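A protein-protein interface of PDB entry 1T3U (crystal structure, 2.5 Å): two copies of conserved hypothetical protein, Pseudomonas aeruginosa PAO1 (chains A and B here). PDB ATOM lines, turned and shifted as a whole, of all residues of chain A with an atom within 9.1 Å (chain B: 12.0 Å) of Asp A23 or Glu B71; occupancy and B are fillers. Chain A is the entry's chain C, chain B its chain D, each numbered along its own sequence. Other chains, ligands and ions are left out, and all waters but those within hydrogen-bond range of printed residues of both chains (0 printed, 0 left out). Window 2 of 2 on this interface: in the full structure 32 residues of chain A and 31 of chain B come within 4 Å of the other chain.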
ATOM      1  N   THR A   6      -7.980  34.446  -7.338  1.00  0.00           N
ATOM      2  CA  THR A   6      -7.066  34.963  -8.397  1.00  0.00           C
ATOM      3  C   THR A   6      -6.567  36.371  -8.093  1.00  0.00           C
ATOM      4  O   THR A   6      -7.114  37.363  -8.587  1.00  0.00           O
ATOM      5  CB  THR A   6      -7.753  34.966  -9.774  1.00  0.00           C
ATOM      6  OG1 THR A   6      -6.935  35.679 -10.717  1.00  0.00           O
ATOM      7  CG2 THR A   6      -9.132  35.617  -9.680  1.00  0.00           C
ATOM      8  N   CYS A  20      -5.546  31.954  -5.119  1.00  0.00           N
ATOM      9  CA  CYS A  20      -5.612  31.796  -3.671  1.00  0.00           C
ATOM     10  C   CYS A  20      -7.013  32.025  -3.113  1.00  0.00           C
ATOM     11  O   CYS A  20      -7.822  32.757  -3.691  1.00  0.00           O
ATOM     12  CB  CYS A  20      -4.663  32.786  -2.993  1.00  0.00           C
ATOM     13  SG  CYS A  20      -5.254  34.513  -3.019  1.00  0.00           S
ATOM     14  N   PRO A  21      -7.318  31.394  -1.969  1.00  0.00           N
ATOM     15  CA  PRO A  21      -8.629  31.551  -1.340  1.00  0.00           C
ATOM     16  C   PRO A  21      -8.853  33.017  -0.982  1.00  0.00           C
ATOM     17  O   PRO A  21      -7.952  33.686  -0.469  1.00  0.00           O
ATOM     18  CB  PRO A  21      -8.520  30.672  -0.100  1.00  0.00           C
ATOM     19  CG  PRO A  21      -7.605  29.582  -0.552  1.00  0.00           C
ATOM     20  CD  PRO A  21      -6.535  30.348  -1.290  1.00  0.00           C
ATOM     21  N   ASP A  22     -10.055  33.506  -1.260  1.00  0.00           N
ATOM     22  CA  ASP A  22     -10.417  34.889  -0.976  1.00  0.00           C
ATOM     23  C   ASP A  22     -10.005  35.310   0.437  1.00  0.00           C
ATOM     24  O   ASP A  22      -9.613  36.455   0.664  1.00  0.00           O
ATOM     25  CB  ASP A  22     -11.928  35.069  -1.151  1.00  0.00           C
ATOM     26  CG  ASP A  22     -12.410  34.649  -2.530  1.00  0.00           C
ATOM     27  OD1 ASP A  22     -12.024  35.307  -3.522  1.00  0.00           O
ATOM     28  OD2 ASP A  22     -13.171  33.658  -2.625  1.00  0.00           O
ATOM     29  N   ASP A  23     -10.080  34.375   1.379  1.00  0.00           N
ATOM     30  CA  ASP A  23      -9.737  34.658   2.768  1.00  0.00           C
ATOM     31  C   ASP A  23      -8.229  34.666   3.006  1.00  0.00           C
ATOM     32  O   ASP A  23      -7.768  34.517   4.137  1.00  0.00           O
ATOM     33  CB  ASP A  23     -10.405  33.632   3.686  1.00  0.00           C
ATOM     34  CG  ASP A  23     -10.703  34.191   5.062  1.00  0.00           C
ATOM     35  OD1 ASP A  23     -11.427  35.210   5.135  1.00  0.00           O
ATOM     36  OD2 ASP A  23     -10.220  33.612   6.062  1.00  0.00           O
ATOM     37  N   GLU A  24      -7.465  34.848   1.936  1.00  0.00           N
ATOM     38  CA  GLU A  24      -6.016  34.882   2.035  1.00  0.00           C
ATOM     39  C   GLU A  24      -5.395  36.070   1.297  1.00  0.00           C
ATOM     40  O   GLU A  24      -4.234  36.399   1.524  1.00  0.00           O
ATOM     41  CB  GLU A  24      -5.434  33.568   1.509  1.00  0.00           C
ATOM     42  CG  GLU A  24      -5.329  32.473   2.560  1.00  0.00           C
ATOM     43  CD  GLU A  24      -4.830  31.149   1.991  1.00  0.00           C
ATOM     44  OE1 GLU A  24      -3.875  31.170   1.184  1.00  0.00           O
ATOM     45  OE2 GLU A  24      -5.382  30.086   2.359  1.00  0.00           O
ATOM     46  N   ARG A  25      -6.175  36.712   0.426  1.00  0.00           N
ATOM     47  CA  ARG A  25      -5.717  37.865  -0.358  1.00  0.00           C
ATOM     48  C   ARG A  25      -4.861  38.827   0.462  1.00  0.00           C
ATOM     49  O   ARG A  25      -3.696  39.064   0.143  1.00  0.00           O
ATOM     50  CB  ARG A  25      -6.910  38.646  -0.912  1.00  0.00           C
ATOM     51  CG  ARG A  25      -7.957  37.799  -1.598  1.00  0.00           C
ATOM     52  CD  ARG A  25      -7.697  37.664  -3.084  1.00  0.00           C
ATOM     53  NE  ARG A  25      -7.840  38.938  -3.782  1.00  0.00           N
ATOM     54  CZ  ARG A  25      -7.942  39.049  -5.102  1.00  0.00           C
ATOM     55  NH1 ARG A  25      -7.919  37.960  -5.863  1.00  0.00           N
ATOM     56  NH2 ARG A  25      -8.068  40.244  -5.662  1.00  0.00           N
ATOM     57  N   ALA A  26      -5.443  39.388   1.516  1.00  0.00           N
ATOM     58  CA  ALA A  26      -4.720  40.328   2.354  1.00  0.00           C
ATOM     59  C   ALA A  26      -3.379  39.781   2.830  1.00  0.00           C
ATOM     60  O   ALA A  26      -2.369  40.461   2.704  1.00  0.00           O
ATOM     61  CB  ALA A  26      -5.571  40.738   3.542  1.00  0.00           C
ATOM     62  N   ASN A  27      -3.360  38.562   3.371  1.00  0.00           N
ATOM     63  CA  ASN A  27      -2.106  37.985   3.856  1.00  0.00           C
ATOM     64  C   ASN A  27      -1.074  37.763   2.762  1.00  0.00           C
ATOM     65  O   ASN A  27       0.114  37.996   2.970  1.00  0.00           O
ATOM     66  CB  ASN A  27      -2.340  36.663   4.588  1.00  0.00           C
ATOM     67  CG  ASN A  27      -2.559  36.855   6.076  1.00  0.00           C
ATOM     68  OD1 ASN A  27      -1.893  37.675   6.717  1.00  0.00           O
ATOM     69  ND2 ASN A  27      -3.484  36.089   6.640  1.00  0.00           N
ATOM     70  N   LEU A  28      -1.518  37.302   1.602  1.00  0.00           N
ATOM     71  CA  LEU A  28      -0.581  37.083   0.525  1.00  0.00           C
ATOM     72  C   LEU A  28      -0.017  38.415   0.012  1.00  0.00           C
ATOM     73  O   LEU A  28       1.160  38.495  -0.360  1.00  0.00           O
ATOM     74  CB  LEU A  28      -1.236  36.275  -0.601  1.00  0.00           C
ATOM     75  CG  LEU A  28      -1.294  34.764  -0.329  1.00  0.00           C
ATOM     76  CD1 LEU A  28      -2.010  34.057  -1.452  1.00  0.00           C
ATOM     77  CD2 LEU A  28       0.118  34.206  -0.182  1.00  0.00           C
ATOM     78  N   LEU A  73       3.100  28.360  16.043  1.00  0.00           N
ATOM     79  CA  LEU A  73       1.757  27.873  15.774  1.00  0.00           C
ATOM     80  C   LEU A  73       1.670  26.397  16.193  1.00  0.00           C
ATOM     81  O   LEU A  73       0.673  25.969  16.771  1.00  0.00           O
ATOM     82  CB  LEU A  73       1.425  28.036  14.286  1.00  0.00           C
ATOM     83  CG  LEU A  73       0.014  27.653  13.828  1.00  0.00           C
ATOM     84  CD1 LEU A  73      -1.025  28.598  14.441  1.00  0.00           C
ATOM     85  CD2 LEU A  73      -0.052  27.711  12.316  1.00  0.00           C
ATOM     86  N   ILE B  62       4.990  28.878  -0.277  1.00  0.00           N
ATOM     87  CA  ILE B  62       5.320  28.558   1.099  1.00  0.00           C
ATOM     88  C   ILE B  62       4.465  29.431   2.023  1.00  0.00           C
ATOM     89  O   ILE B  62       4.049  28.991   3.100  1.00  0.00           O
ATOM     90  CB  ILE B  62       6.807  28.780   1.365  1.00  0.00           C
ATOM     91  CG1 ILE B  62       7.624  27.793   0.505  1.00  0.00           C
ATOM     92  CG2 ILE B  62       7.103  28.610   2.838  1.00  0.00           C
ATOM     93  CD1 ILE B  62       9.137  28.029   0.536  1.00  0.00           C
ATOM     94  N   THR B  63       4.182  30.660   1.597  1.00  0.00           N
ATOM     95  CA  THR B  63       3.351  31.541   2.402  1.00  0.00           C
ATOM     96  C   THR B  63       1.935  30.966   2.442  1.00  0.00           C
ATOM     97  O   THR B  63       1.356  30.756   3.514  1.00  0.00           O
ATOM     98  CB  THR B  63       3.306  32.957   1.821  1.00  0.00           C
ATOM     99  OG1 THR B  63       4.598  33.556   1.944  1.00  0.00           O
ATOM    100  CG2 THR B  63       2.297  33.815   2.581  1.00  0.00           C
ATOM    101  N   HIS B  64       1.388  30.714   1.265  1.00  0.00           N
ATOM    102  CA  HIS B  64       0.064  30.145   1.157  1.00  0.00           C
ATOM    103  C   HIS B  64      -0.041  28.856   1.981  1.00  0.00           C
ATOM    104  O   HIS B  64      -1.067  28.597   2.606  1.00  0.00           O
ATOM    105  CB  HIS B  64      -0.234  29.840  -0.304  1.00  0.00           C
ATOM    106  CG  HIS B  64      -1.409  28.934  -0.503  1.00  0.00           C
ATOM    107  ND1 HIS B  64      -2.706  29.392  -0.545  1.00  0.00           N
ATOM    108  CD2 HIS B  64      -1.476  27.591  -0.691  1.00  0.00           C
ATOM    109  CE1 HIS B  64      -3.523  28.373  -0.755  1.00  0.00           C
ATOM    110  NE2 HIS B  64      -2.800  27.270  -0.847  1.00  0.00           N
ATOM    111  N   ASP B  65       1.024  28.055   1.971  1.00  0.00           N
ATOM    112  CA  ASP B  65       1.049  26.790   2.699  1.00  0.00           C
ATOM    113  C   ASP B  65       0.805  26.954   4.194  1.00  0.00           C
ATOM    114  O   ASP B  65       0.015  26.215   4.771  1.00  0.00           O
ATOM    115  CB  ASP B  65       2.384  26.072   2.469  1.00  0.00           C
ATOM    116  CG  ASP B  65       2.345  25.124   1.273  1.00  0.00           C
ATOM    117  OD1 ASP B  65       1.448  25.287   0.417  1.00  0.00           O
ATOM    118  OD2 ASP B  65       3.213  24.221   1.185  1.00  0.00           O
ATOM    119  N   LEU B  66       1.485  27.906   4.825  1.00  0.00           N
ATOM    120  CA  LEU B  66       1.310  28.132   6.253  1.00  0.00           C
ATOM    121  C   LEU B  66      -0.073  28.712   6.545  1.00  0.00           C
ATOM    122  O   LEU B  66      -0.695  28.374   7.554  1.00  0.00           O
ATOM    123  CB  LEU B  66       2.403  29.071   6.784  1.00  0.00           C
ATOM    124  CG  LEU B  66       2.401  29.524   8.259  1.00  0.00           C
ATOM    125  CD1 LEU B  66       3.825  29.825   8.691  1.00  0.00           C
ATOM    126  CD2 LEU B  66       1.521  30.761   8.453  1.00  0.00           C
ATOM    127  N   LEU B  67      -0.552  29.587   5.663  1.00  0.00           N
ATOM    128  CA  LEU B  67      -1.863  30.196   5.841  1.00  0.00           C
ATOM    129  C   LEU B  67      -2.932  29.119   5.843  1.00  0.00           C
ATOM    130  O   LEU B  67      -3.785  29.089   6.725  1.00  0.00           O
ATOM    131  CB  LEU B  67      -2.150  31.189   4.721  1.00  0.00           C
ATOM    132  CG  LEU B  67      -1.287  32.443   4.671  1.00  0.00           C
ATOM    133  CD1 LEU B  67      -1.665  33.262   3.445  1.00  0.00           C
ATOM    134  CD2 LEU B  67      -1.473  33.248   5.951  1.00  0.00           C
ATOM    135  N   HIS B  68      -2.861  28.241   4.847  1.00  0.00           N
ATOM    136  CA  HIS B  68      -3.801  27.146   4.669  1.00  0.00           C
ATOM    137  C   HIS B  68      -3.677  26.157   5.794  1.00  0.00           C
ATOM    138  O   HIS B  68      -4.633  25.469   6.131  1.00  0.00           O
ATOM    139  CB  HIS B  68      -3.522  26.431   3.356  1.00  0.00           C
ATOM    140  CG  HIS B  68      -4.594  25.472   2.957  1.00  0.00           C
ATOM    141  ND1 HIS B  68      -4.396  24.109   2.905  1.00  0.00           N
ATOM    142  CD2 HIS B  68      -5.883  25.683   2.603  1.00  0.00           C
ATOM    143  CE1 HIS B  68      -5.520  23.522   2.532  1.00  0.00           C
ATOM    144  NE2 HIS B  68      -6.437  24.454   2.344  1.00  0.00           N
ATOM    145  N   ARG B  69      -2.482  26.073   6.358  1.00  0.00           N
ATOM    146  CA  ARG B  69      -2.235  25.169   7.463  1.00  0.00           C
ATOM    147  C   ARG B  69      -2.938  25.738   8.672  1.00  0.00           C
ATOM    148  O   ARG B  69      -3.442  25.004   9.513  1.00  0.00           O
ATOM    149  CB  ARG B  69      -0.741  25.081   7.760  1.00  0.00           C
ATOM    150  CG  ARG B  69      -0.400  24.243   8.980  1.00  0.00           C
ATOM    151  CD  ARG B  69       0.082  22.856   8.584  1.00  0.00           C
ATOM    152  NE  ARG B  69       0.273  21.991   9.748  1.00  0.00           N
ATOM    153  CZ  ARG B  69       1.112  22.246  10.750  1.00  0.00           C
ATOM    154  NH1 ARG B  69       1.852  23.348  10.745  1.00  0.00           N
ATOM    155  NH2 ARG B  69       1.214  21.397  11.763  1.00  0.00           N
ATOM    156  N   LYS B  70      -2.969  27.061   8.752  1.00  0.00           N
ATOM    157  CA  LYS B  70      -3.596  27.722   9.877  1.00  0.00           C
ATOM    158  C   LYS B  70      -5.122  27.683   9.766  1.00  0.00           C
ATOM    159  O   LYS B  70      -5.803  27.249  10.690  1.00  0.00           O
ATOM    160  CB  LYS B  70      -3.095  29.166   9.970  1.00  0.00           C
ATOM    161  CG  LYS B  70      -3.262  29.800  11.339  1.00  0.00           C
ATOM    162  CD  LYS B  70      -4.112  31.038  11.267  1.00  0.00           C
ATOM    163  CE  LYS B  70      -4.510  31.516  12.654  1.00  0.00           C
ATOM    164  NZ  LYS B  70      -5.565  32.581  12.590  1.00  0.00           N
ATOM    165  N   GLU B  71      -5.657  28.124   8.633  1.00  0.00           N
ATOM    166  CA  GLU B  71      -7.102  28.131   8.447  1.00  0.00           C
ATOM    167  C   GLU B  71      -7.653  26.725   8.713  1.00  0.00           C
ATOM    168  O   GLU B  71      -8.691  26.563   9.349  1.00  0.00           O
ATOM    169  CB  GLU B  71      -7.443  28.593   7.025  1.00  0.00           C
ATOM    170  CG  GLU B  71      -8.853  29.185   6.848  1.00  0.00           C
ATOM    171  CD  GLU B  71      -9.107  30.442   7.700  1.00  0.00           C
ATOM    172  OE1 GLU B  71      -8.273  31.387   7.675  1.00  0.00           O
ATOM    173  OE2 GLU B  71     -10.156  30.486   8.384  1.00  0.00           O
ATOM    174  N   ARG B  72      -6.937  25.710   8.253  1.00  0.00           N
ATOM    175  CA  ARG B  72      -7.360  24.329   8.442  1.00  0.00           C
ATOM    176  C   ARG B  72      -7.336  23.926   9.906  1.00  0.00           C
ATOM    177  O   ARG B  72      -8.071  23.046  10.329  1.00  0.00           O
ATOM    178  CB  ARG B  72      -6.451  23.387   7.650  1.00  0.00           C
ATOM    179  CG  ARG B  72      -6.852  21.923   7.710  1.00  0.00           C
ATOM    180  CD  ARG B  72      -8.142  21.672   6.941  1.00  0.00           C
ATOM    181  NE  ARG B  72      -7.952  21.794   5.501  1.00  0.00           N
ATOM    182  CZ  ARG B  72      -8.945  21.761   4.612  1.00  0.00           C
ATOM    183  NH1 ARG B  72     -10.200  21.613   5.024  1.00  0.00           N
ATOM    184  NH2 ARG B  72      -8.687  21.870   3.310  1.00  0.00           N
ATOM    185  N   LEU B  73      -6.483  24.568  10.682  1.00  0.00           N
ATOM    186  CA  LEU B  73      -6.377  24.245  12.085  1.00  0.00           C
ATOM    187  C   LEU B  73      -7.448  25.003  12.865  1.00  0.00           C
ATOM    188  O   LEU B  73      -7.911  24.557  13.916  1.00  0.00           O
ATOM    189  CB  LEU B  73      -4.978  24.607  12.561  1.00  0.00           C
ATOM    190  CG  LEU B  73      -4.455  24.005  13.859  1.00  0.00           C
ATOM    191  CD1 LEU B  73      -2.942  23.940  13.777  1.00  0.00           C
ATOM    192  CD2 LEU B  73      -4.912  24.830  15.053  1.00  0.00           C
ATOM    193  N   ASP B  74      -7.844  26.156  12.348  1.00  0.00           N
ATOM    194  CA  ASP B  74      -8.879  26.940  12.998  1.00  0.00           C
ATOM    195  C   ASP B  74     -10.231  26.268  12.716  1.00  0.00           C
ATOM    196  O   ASP B  74     -11.159  26.353  13.517  1.00  0.00           O
ATOM    197  CB  ASP B  74      -8.866  28.380  12.466  1.00  0.00           C
ATOM    198  CG  ASP B  74      -7.650  29.182  12.940  1.00  0.00           C
ATOM    199  OD1 ASP B  74      -7.439  30.301  12.416  1.00  0.00           O
ATOM    200  OD2 ASP B  74      -6.907  28.710  13.835  1.00  0.00           O
ATOM    201  N   GLN B  75     -10.324  25.590  11.574  1.00  0.00           N
ATOM    202  CA  GLN B  75     -11.549  24.900  11.196  1.00  0.00           C
ATOM    203  C   GLN B  75     -11.726  23.582  11.933  1.00  0.00           C
ATOM    204  O   GLN B  75     -12.847  23.108  12.122  1.00  0.00           O
ATOM    205  CB  GLN B  75     -11.592  24.675   9.684  1.00  0.00           C
ATOM    206  CG  GLN B  75     -11.866  25.960   8.932  1.00  0.00           C
ATOM    207  CD  GLN B  75     -11.914  25.782   7.430  1.00  0.00           C
ATOM    208  OE1 GLN B  75     -11.959  26.770   6.683  1.00  0.00           O
ATOM    209  NE2 GLN B  75     -11.907  24.527   6.971  1.00  0.00           N
ATOM    210  N   GLU B  76     -10.620  22.983  12.348  1.00  0.00           N
ATOM    211  CA  GLU B  76     -10.704  21.747  13.088  1.00  0.00           C
ATOM    212  C   GLU B  76     -11.123  22.065  14.513  1.00  0.00           C
ATOM    213  O   GLU B  76     -11.857  21.309  15.125  1.00  0.00           O
ATOM    214  CB  GLU B  76      -9.360  21.028  13.085  1.00  0.00           C
ATOM    215  CG  GLU B  76      -9.184  20.076  11.922  1.00  0.00           C
ATOM    216  CD  GLU B  76     -10.045  18.822  12.043  1.00  0.00           C
ATOM    217  OE1 GLU B  76      -9.831  17.873  11.249  1.00  0.00           O
ATOM    218  OE2 GLU B  76     -10.933  18.779  12.927  1.00  0.00           O
ATOM    219  N   SER B  77     -10.669  23.197  15.031  1.00  0.00           N
ATOM    220  CA  SER B  77     -11.012  23.581  16.390  1.00  0.00           C
ATOM    221  C   SER B  77     -12.456  24.011  16.470  1.00  0.00           C
ATOM    222  O   SER B  77     -13.153  23.759  17.459  1.00  0.00           O
ATOM    223  CB  SER B  77     -10.124  24.725  16.857  1.00  0.00           C
ATOM    224  OG  SER B  77      -8.783  24.277  16.948  1.00  0.00           O
ATOM    225  N   SER B  78     -12.889  24.667  15.404  1.00  0.00           N
ATOM    226  CA  SER B  78     -14.241  25.171  15.279  1.00  0.00           C
ATOM    227  C   SER B  78     -15.230  24.015  15.277  1.00  0.00           C
ATOM    228  O   SER B  78     -16.266  24.072  15.930  1.00  0.00           O
ATOM    229  CB  SER B  78     -14.353  25.971  13.984  1.00  0.00           C
ATOM    230  OG  SER B  78     -15.685  26.401  13.767  1.00  0.00           O
ATOM    231  N   SER B  79     -14.888  22.954  14.563  1.00  0.00           N
ATOM    232  CA  SER B  79     -15.771  21.812  14.490  1.00  0.00           C
ATOM    233  C   SER B  79     -15.771  21.026  15.805  1.00  0.00           C
ATOM    234  O   SER B  79     -16.797  20.494  16.218  1.00  0.00           O
ATOM    235  CB  SER B  79     -15.387  20.925  13.304  1.00  0.00           C
ATOM    236  OG  SER B  79     -14.469  19.925  13.676  1.00  0.00           O
ATOM    237  N   THR B  80     -14.620  20.970  16.462  1.00  0.00           N
ATOM    238  CA  THR B  80     -14.491  20.288  17.742  1.00  0.00           C
ATOM    239  C   THR B  80     -15.311  21.037  18.783  1.00  0.00           C
ATOM    240  O   THR B  80     -15.837  20.455  19.720  1.00  0.00           O
ATOM    241  CB  THR B  80     -13.015  20.246  18.191  1.00  0.00           C
ATOM    242  OG1 THR B  80     -12.290  19.400  17.300  1.00  0.00           O
ATOM    243  CG2 THR B  80     -12.878  19.717  19.611  1.00  0.00           C
ATOM    244  N   ARG B  81     -15.392  22.344  18.636  1.00  0.00           N
ATOM    245  CA  ARG B  81     -16.185  23.119  19.559  1.00  0.00           C
ATOM    246  C   ARG B  81     -17.670  22.807  19.374  1.00  0.00           C
ATOM    247  O   ARG B  81     -18.419  22.737  20.344  1.00  0.00           O
ATOM    248  CB  ARG B  81     -15.957  24.615  19.341  1.00  0.00           C
ATOM    249  CG  ARG B  81     -14.749  25.181  20.076  1.00  0.00           C
ATOM    250  CD  ARG B  81     -15.108  26.508  20.723  1.00  0.00           C
ATOM    251  NE  ARG B  81     -14.994  27.630  19.807  1.00  0.00           N
ATOM    252  CZ  ARG B  81     -15.600  28.802  19.972  1.00  0.00           C
ATOM    253  NH1 ARG B  81     -16.384  29.005  21.019  1.00  0.00           N
ATOM    254  NH2 ARG B  81     -15.389  29.784  19.102  1.00  0.00           N
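Position printed for both chains: 73.
Of the 9 pairs that touch across the chains among the printed residues, none has its exchanged pair printed and touching as well.
The side-chain carboxylate of Glu A24 sits at hydrogen-bond distance from a ring nitrogen (ND1) of His B64.
The side-chain carboxylate (OD2) of Asp A23 sits close to the side-chain carboxylate (OE1) of Glu B71.
Among the printed residues, merely in contact across the chains: Pro A21 with His B64 (3.6 Å), Glu A24 with Leu B67 (3.8 Å), Glu A24 with His B68 (3.99 Å), Asn A27 with Leu B67 (3.5 Å), Leu A28 with Thr B63 (3.5 Å), Leu A28 with His B64 (3.99 Å) and Leu A73 with Lys B70 (3.95 Å).
Of chain B, only Glu B71 comes within 4 Å of Asp A23.
Of chain A, only Asp A23 comes within 4 Å of Glu B71.
Pro A21 touches just one residue of chain B: His B64 (3.6 Å).
Of the printed residues of chain A, Leu B67 touches Glu A24 and Asn A27.
Printed residues of chain A within 4 Å of His B64: Pro A21, Glu A24 and Leu A28.
Of the printed residues of chain B, Leu A28 touches Thr B63 and His B64.
Of the printed residues of chain A, Thr B63 touches Leu A28.
The nearest residue of chain B that does not touch Asp A23 is Leu B67 (6.3 Å).
The nearest printed residue of chain B that does not touch Asn A27 is Thr B63 (4.7 Å).
Hydrophobic or aromatic side chains of chain B that line the printed part of chain A: His B64 and Leu B67.
Of the 11 printed residues of chain A, 6 touch a printed residue of chain B.
Hydrophobic or aromatic side chains of chain A within 4 Å of the printed part of chain B: Pro A21, Leu A28 and Leu A73.
The side-chain carboxylate of Asp B74 is in salt-bridge range of the side-chain amino group of Lys B70 (3.0 Å).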
